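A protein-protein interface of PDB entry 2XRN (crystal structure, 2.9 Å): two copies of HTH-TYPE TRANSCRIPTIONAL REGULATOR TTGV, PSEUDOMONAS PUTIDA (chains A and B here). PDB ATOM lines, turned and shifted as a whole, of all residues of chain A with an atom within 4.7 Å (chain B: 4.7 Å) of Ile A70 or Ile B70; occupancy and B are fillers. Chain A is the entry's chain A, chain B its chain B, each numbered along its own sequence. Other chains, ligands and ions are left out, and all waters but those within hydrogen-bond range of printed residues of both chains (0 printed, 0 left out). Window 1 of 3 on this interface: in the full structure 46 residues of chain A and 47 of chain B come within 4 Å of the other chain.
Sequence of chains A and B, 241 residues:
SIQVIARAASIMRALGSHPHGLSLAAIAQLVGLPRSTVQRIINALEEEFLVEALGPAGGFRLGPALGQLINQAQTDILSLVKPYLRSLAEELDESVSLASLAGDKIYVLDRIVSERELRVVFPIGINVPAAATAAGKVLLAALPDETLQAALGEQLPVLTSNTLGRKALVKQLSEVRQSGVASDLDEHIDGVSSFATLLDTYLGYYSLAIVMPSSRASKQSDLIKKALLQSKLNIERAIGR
N of Gly A67 sits at hydrogen-bond distance from O of Leu B203.
The side-chain amide oxygen of Gln B74 lies close to the side-chain amide oxygen of Gln A74 (3.2 Å).
O of Leu A203 is in hydrogen-bond range of N of Gly B67 (3.2 Å).
O of Gly A67 lies close to ND2 of Asn A71, at 3.5 Å.
Among the printed residues, pairs that only touch across the chains: Leu A66 with Ile B70 (3.6 Å), Ile A70 with Leu B66 (3.7 Å), Asn A71 with Gln B74 (3.9 Å), Gln A74 with Asn B71 (3.9 Å) and Ile A70 with Ile B70 (3.99 Å).
Printed residues of chain B within 4 Å of Ile A70: Leu B66 (3.7 Å) and Ile B70 (3.99 Å).
Of the printed residues of chain A, Leu B66 touches Ile A70.
Printed residues of chain A within 4 Å of Leu B203: Gly A67.
Leu A69 touches none of the printed residues of chain B.
The nearest printed residue of chain B that does not touch Ile A70 is Gln B74 (4.1 Å).
The nearest printed residue of chain A that does not touch Ile B70 is Gln A74 (4.1 Å).
The nearest printed residue of chain A that does not touch Leu B203 is Gln A68 (4.2 Å).
Of the 10 printed residues of chain A, 6 touch a printed residue of chain B.
Along chain A the printed residues that touch a printed residue of chain B span positions 66 to 203.
Among the printed residues, no Asp or Glu carboxylate lies within 4 Å of a Lys or Arg side-chain nitrogen of the other chain.
Leu A66 touches Ile B70, and with the chains exchanged Ile A70 touches Leu B66.
Gly A67 touches Leu B203, and with the chains exchanged Leu A203 touches Gly B67.
Asn A71 touches Gln B74, and with the chains exchanged Gln A74 touches Asn B71.
Gln B74 touches its own counterpart, Gln A74.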
ATOM      1  N   LEU A  66     -21.136  -6.304   3.828  1.00  0.00           N
ATOM      2  CA  LEU A  66     -20.794  -7.092   2.650  1.00  0.00           C
ATOM      3  C   LEU A  66     -21.944  -7.216   1.659  1.00  0.00           C
ATOM      4  O   LEU A  66     -21.829  -6.780   0.511  1.00  0.00           O
ATOM      5  CB  LEU A  66     -20.320  -8.478   3.059  1.00  0.00           C
ATOM      6  CG  LEU A  66     -18.815  -8.652   2.921  1.00  0.00           C
ATOM      7  CD1 LEU A  66     -18.128  -7.359   3.272  1.00  0.00           C
ATOM      8  CD2 LEU A  66     -18.329  -9.791   3.798  1.00  0.00           C
ATOM      9  N   GLY A  67     -23.049  -7.810   2.101  1.00  0.00           N
ATOM     10  CA  GLY A  67     -24.217  -7.959   1.254  1.00  0.00           C
ATOM     11  C   GLY A  67     -24.491  -6.716   0.433  1.00  0.00           C
ATOM     12  O   GLY A  67     -24.479  -6.752  -0.802  1.00  0.00           O
ATOM     13  N   GLN A  68     -24.686  -5.599   1.119  1.00  0.00           N
ATOM     14  CA  GLN A  68     -25.126  -4.373   0.467  1.00  0.00           C
ATOM     15  C   GLN A  68     -24.112  -3.818  -0.539  1.00  0.00           C
ATOM     16  O   GLN A  68     -24.474  -3.058  -1.442  1.00  0.00           O
ATOM     17  CB  GLN A  68     -25.498  -3.333   1.520  1.00  0.00           C
ATOM     18  CG  GLN A  68     -25.789  -3.950   2.896  1.00  0.00           C
ATOM     19  CD  GLN A  68     -26.744  -5.148   2.841  1.00  0.00           C
ATOM     20  OE1 GLN A  68     -27.467  -5.351   1.863  1.00  0.00           O
ATOM     21  NE2 GLN A  68     -26.742  -5.947   3.900  1.00  0.00           N
ATOM     22  N   LEU A  69     -22.846  -4.204  -0.387  1.00  0.00           N
ATOM     23  CA  LEU A  69     -21.820  -3.848  -1.360  1.00  0.00           C
ATOM     24  C   LEU A  69     -22.004  -4.632  -2.646  1.00  0.00           C
ATOM     25  O   LEU A  69     -21.993  -4.070  -3.741  1.00  0.00           O
ATOM     26  CB  LEU A  69     -20.430  -4.151  -0.812  1.00  0.00           C
ATOM     27  CG  LEU A  69     -19.910  -3.238   0.287  1.00  0.00           C
ATOM     28  CD1 LEU A  69     -18.485  -3.625   0.649  1.00  0.00           C
ATOM     29  CD2 LEU A  69     -19.975  -1.807  -0.187  1.00  0.00           C
ATOM     30  N   ILE A  70     -22.177  -5.942  -2.492  1.00  0.00           N
ATOM     31  CA  ILE A  70     -22.179  -6.862  -3.617  1.00  0.00           C
ATOM     32  C   ILE A  70     -23.528  -6.962  -4.335  1.00  0.00           C
ATOM     33  O   ILE A  70     -23.593  -6.899  -5.568  1.00  0.00           O
ATOM     34  CB  ILE A  70     -21.767  -8.261  -3.149  1.00  0.00           C
ATOM     35  CG1 ILE A  70     -20.267  -8.451  -3.313  1.00  0.00           C
ATOM     36  CG2 ILE A  70     -22.482  -9.309  -3.947  1.00  0.00           C
ATOM     37  CD1 ILE A  70     -19.827  -8.395  -4.759  1.00  0.00           C
ATOM     38  N   ASN A  71     -24.599  -7.112  -3.558  1.00  0.00           N
ATOM     39  CA  ASN A  71     -25.917  -7.418  -4.107  1.00  0.00           C
ATOM     40  C   ASN A  71     -26.292  -6.871  -5.482  1.00  0.00           C
ATOM     41  O   ASN A  71     -26.480  -7.635  -6.424  1.00  0.00           O
ATOM     42  CB  ASN A  71     -27.029  -7.000  -3.142  1.00  0.00           C
ATOM     43  CG  ASN A  71     -27.201  -7.977  -1.990  1.00  0.00           C
ATOM     44  OD1 ASN A  71     -26.754  -9.126  -2.057  1.00  0.00           O
ATOM     45  ND2 ASN A  71     -27.856  -7.526  -0.926  1.00  0.00           N
ATOM     46  N   GLN A  72     -26.388  -5.552  -5.595  1.00  0.00           N
ATOM     47  CA  GLN A  72     -26.771  -4.924  -6.854  1.00  0.00           C
ATOM     48  C   GLN A  72     -25.838  -5.418  -7.958  1.00  0.00           C
ATOM     49  O   GLN A  72     -26.291  -6.004  -8.944  1.00  0.00           O
ATOM     50  CB  GLN A  72     -26.681  -3.406  -6.718  1.00  0.00           C
ATOM     51  CG  GLN A  72     -27.251  -2.895  -5.411  1.00  0.00           C
ATOM     52  CD  GLN A  72     -28.002  -1.598  -5.574  1.00  0.00           C
ATOM     53  OE1 GLN A  72     -28.236  -1.136  -6.694  1.00  0.00           O
ATOM     54  NE2 GLN A  72     -28.395  -1.000  -4.455  1.00  0.00           N
ATOM     55  N   ALA A  73     -24.536  -5.205  -7.783  1.00  0.00           N
ATOM     56  CA  ALA A  73     -23.566  -5.619  -8.791  1.00  0.00           C
ATOM     57  C   ALA A  73     -23.878  -7.026  -9.260  1.00  0.00           C
ATOM     58  O   ALA A  73     -24.171  -7.246 -10.437  1.00  0.00           O
ATOM     59  CB  ALA A  73     -22.154  -5.542  -8.244  1.00  0.00           C
ATOM     60  N   GLN A  74     -23.836  -7.976  -8.330  1.00  0.00           N
ATOM     61  CA  GLN A  74     -24.180  -9.360  -8.639  1.00  0.00           C
ATOM     62  C   GLN A  74     -25.514  -9.501  -9.381  1.00  0.00           C
ATOM     63  O   GLN A  74     -25.575 -10.095 -10.460  1.00  0.00           O
ATOM     64  CB  GLN A  74     -24.201 -10.202  -7.366  1.00  0.00           C
ATOM     65  CG  GLN A  74     -22.853 -10.785  -6.987  1.00  0.00           C
ATOM     66  CD  GLN A  74     -22.924 -11.663  -5.749  1.00  0.00           C
ATOM     67  OE1 GLN A  74     -23.867 -11.567  -4.960  1.00  0.00           O
ATOM     68  NE2 GLN A  74     -21.924 -12.518  -5.571  1.00  0.00           N
ATOM     69  N   LEU A 203     -16.427  -8.975 -11.555  1.00  0.00           N
ATOM     70  CA  LEU A 203     -16.899  -9.239 -10.205  1.00  0.00           C
ATOM     71  C   LEU A 203     -16.347 -10.557  -9.670  1.00  0.00           C
ATOM     72  O   LEU A 203     -16.567 -10.906  -8.511  1.00  0.00           O
ATOM     73  CB  LEU A 203     -18.427  -9.241 -10.177  1.00  0.00           C
ATOM     74  CG  LEU A 203     -19.134  -8.977  -8.849  1.00  0.00           C
ATOM     75  CD1 LEU A 203     -18.620  -7.709  -8.173  1.00  0.00           C
ATOM     76  CD2 LEU A 203     -20.633  -8.884  -9.094  1.00  0.00           C
ATOM     77  N   LEU B  66     -13.887  -9.203  -4.693  1.00  0.00           N
ATOM     78  CA  LEU B  66     -15.203  -9.208  -4.065  1.00  0.00           C
ATOM     79  C   LEU B  66     -15.875 -10.574  -4.102  1.00  0.00           C
ATOM     80  O   LEU B  66     -16.171 -11.155  -3.058  1.00  0.00           O
ATOM     81  CB  LEU B  66     -16.109  -8.172  -4.720  1.00  0.00           C
ATOM     82  CG  LEU B  66     -16.319  -6.939  -3.853  1.00  0.00           C
ATOM     83  CD1 LEU B  66     -15.043  -6.634  -3.097  1.00  0.00           C
ATOM     84  CD2 LEU B  66     -16.745  -5.760  -4.707  1.00  0.00           C
ATOM     85  N   GLY B  67     -16.117 -11.081  -5.307  1.00  0.00           N
ATOM     86  CA  GLY B  67     -16.734 -12.382  -5.468  1.00  0.00           C
ATOM     87  C   GLY B  67     -16.183 -13.394  -4.485  1.00  0.00           C
ATOM     88  O   GLY B  67     -16.913 -13.943  -3.657  1.00  0.00           O
ATOM     89  N   GLN B  68     -14.876 -13.606  -4.545  1.00  0.00           N
ATOM     90  CA  GLN B  68     -14.245 -14.674  -3.782  1.00  0.00           C
ATOM     91  C   GLN B  68     -14.362 -14.491  -2.268  1.00  0.00           C
ATOM     92  O   GLN B  68     -14.259 -15.460  -1.513  1.00  0.00           O
ATOM     93  CB  GLN B  68     -12.789 -14.824  -4.215  1.00  0.00           C
ATOM     94  CG  GLN B  68     -12.510 -14.231  -5.604  1.00  0.00           C
ATOM     95  CD  GLN B  68     -13.529 -14.649  -6.671  1.00  0.00           C
ATOM     96  OE1 GLN B  68     -14.263 -15.626  -6.511  1.00  0.00           O
ATOM     97  NE2 GLN B  68     -13.573 -13.898  -7.767  1.00  0.00           N
ATOM     98  N   LEU B  69     -14.589 -13.254  -1.831  1.00  0.00           N
ATOM     99  CA  LEU B  69     -14.844 -12.975  -0.420  1.00  0.00           C
ATOM    100  C   LEU B  69     -16.223 -13.463  -0.022  1.00  0.00           C
ATOM    101  O   LEU B  69     -16.390 -14.144   0.992  1.00  0.00           O
ATOM    102  CB  LEU B  69     -14.771 -11.475  -0.148  1.00  0.00           C
ATOM    103  CG  LEU B  69     -13.386 -10.842  -0.159  1.00  0.00           C
ATOM    104  CD1 LEU B  69     -13.485  -9.376   0.225  1.00  0.00           C
ATOM    105  CD2 LEU B  69     -12.482 -11.590   0.796  1.00  0.00           C
ATOM    106  N   ILE B  70     -17.207 -13.103  -0.839  1.00  0.00           N
ATOM    107  CA  ILE B  70     -18.605 -13.322  -0.509  1.00  0.00           C
ATOM    108  C   ILE B  70     -19.165 -14.705  -0.857  1.00  0.00           C
ATOM    109  O   ILE B  70     -19.947 -15.279  -0.090  1.00  0.00           O
ATOM    110  CB  ILE B  70     -19.488 -12.303  -1.242  1.00  0.00           C
ATOM    111  CG1 ILE B  70     -19.728 -11.082  -0.364  1.00  0.00           C
ATOM    112  CG2 ILE B  70     -20.810 -12.916  -1.599  1.00  0.00           C
ATOM    113  CD1 ILE B  70     -20.508 -11.402   0.886  1.00  0.00           C
ATOM    114  N   ASN B  71     -18.756 -15.235  -2.007  1.00  0.00           N
ATOM    115  CA  ASN B  71     -19.361 -16.444  -2.560  1.00  0.00           C
ATOM    116  C   ASN B  71     -19.702 -17.532  -1.543  1.00  0.00           C
ATOM    117  O   ASN B  71     -20.875 -17.792  -1.279  1.00  0.00           O
ATOM    118  CB  ASN B  71     -18.476 -17.050  -3.652  1.00  0.00           C
ATOM    119  CG  ASN B  71     -18.628 -16.340  -4.990  1.00  0.00           C
ATOM    120  OD1 ASN B  71     -19.602 -15.621  -5.223  1.00  0.00           O
ATOM    121  ND2 ASN B  71     -17.664 -16.549  -5.880  1.00  0.00           N
ATOM    122  N   GLN B  72     -18.681 -18.158  -0.972  1.00  0.00           N
ATOM    123  CA  GLN B  72     -18.891 -19.234  -0.009  1.00  0.00           C
ATOM    124  C   GLN B  72     -19.925 -18.818   1.036  1.00  0.00           C
ATOM    125  O   GLN B  72     -20.979 -19.447   1.167  1.00  0.00           O
ATOM    126  CB  GLN B  72     -17.568 -19.595   0.658  1.00  0.00           C
ATOM    127  CG  GLN B  72     -16.409 -19.638  -0.315  1.00  0.00           C
ATOM    128  CD  GLN B  72     -15.444 -20.765  -0.026  1.00  0.00           C
ATOM    129  OE1 GLN B  72     -15.705 -21.624   0.818  1.00  0.00           O
ATOM    130  NE2 GLN B  72     -14.320 -20.772  -0.733  1.00  0.00           N
ATOM    131  N   ALA B  73     -19.637 -17.744   1.763  1.00  0.00           N
ATOM    132  CA  ALA B  73     -20.556 -17.280   2.796  1.00  0.00           C
ATOM    133  C   ALA B  73     -21.986 -17.296   2.267  1.00  0.00           C
ATOM    134  O   ALA B  73     -22.841 -18.009   2.791  1.00  0.00           O
ATOM    135  CB  ALA B  73     -20.172 -15.890   3.272  1.00  0.00           C
ATOM    136  N   GLN B  74     -22.232 -16.527   1.212  1.00  0.00           N
ATOM    137  CA  GLN B  74     -23.545 -16.483   0.584  1.00  0.00           C
ATOM    138  C   GLN B  74     -24.088 -17.874   0.267  1.00  0.00           C
ATOM    139  O   GLN B  74     -25.193 -18.234   0.693  1.00  0.00           O
ATOM    140  CB  GLN B  74     -23.507 -15.636  -0.687  1.00  0.00           C
ATOM    141  CG  GLN B  74     -23.779 -14.157  -0.454  1.00  0.00           C
ATOM    142  CD  GLN B  74     -23.773 -13.346  -1.738  1.00  0.00           C
ATOM    143  OE1 GLN B  74     -23.243 -13.784  -2.761  1.00  0.00           O
ATOM    144  NE2 GLN B  74     -24.359 -12.156  -1.688  1.00  0.00           N
ATOM    145  N   LEU B 203     -24.846 -11.570   7.141  1.00  0.00           N
ATOM    146  CA  LEU B 203     -24.293 -11.244   5.837  1.00  0.00           C
ATOM    147  C   LEU B 203     -25.066 -10.107   5.170  1.00  0.00           C
ATOM    148  O   LEU B 203     -24.686  -9.626   4.105  1.00  0.00           O
ATOM    149  CB  LEU B 203     -24.289 -12.490   4.951  1.00  0.00           C
ATOM    150  CG  LEU B 203     -23.313 -12.554   3.777  1.00  0.00           C
ATOM    151  CD1 LEU B 203     -21.887 -12.233   4.212  1.00  0.00           C
ATOM    152  CD2 LEU B 203     -23.383 -13.931   3.141  1.00  0.00           C
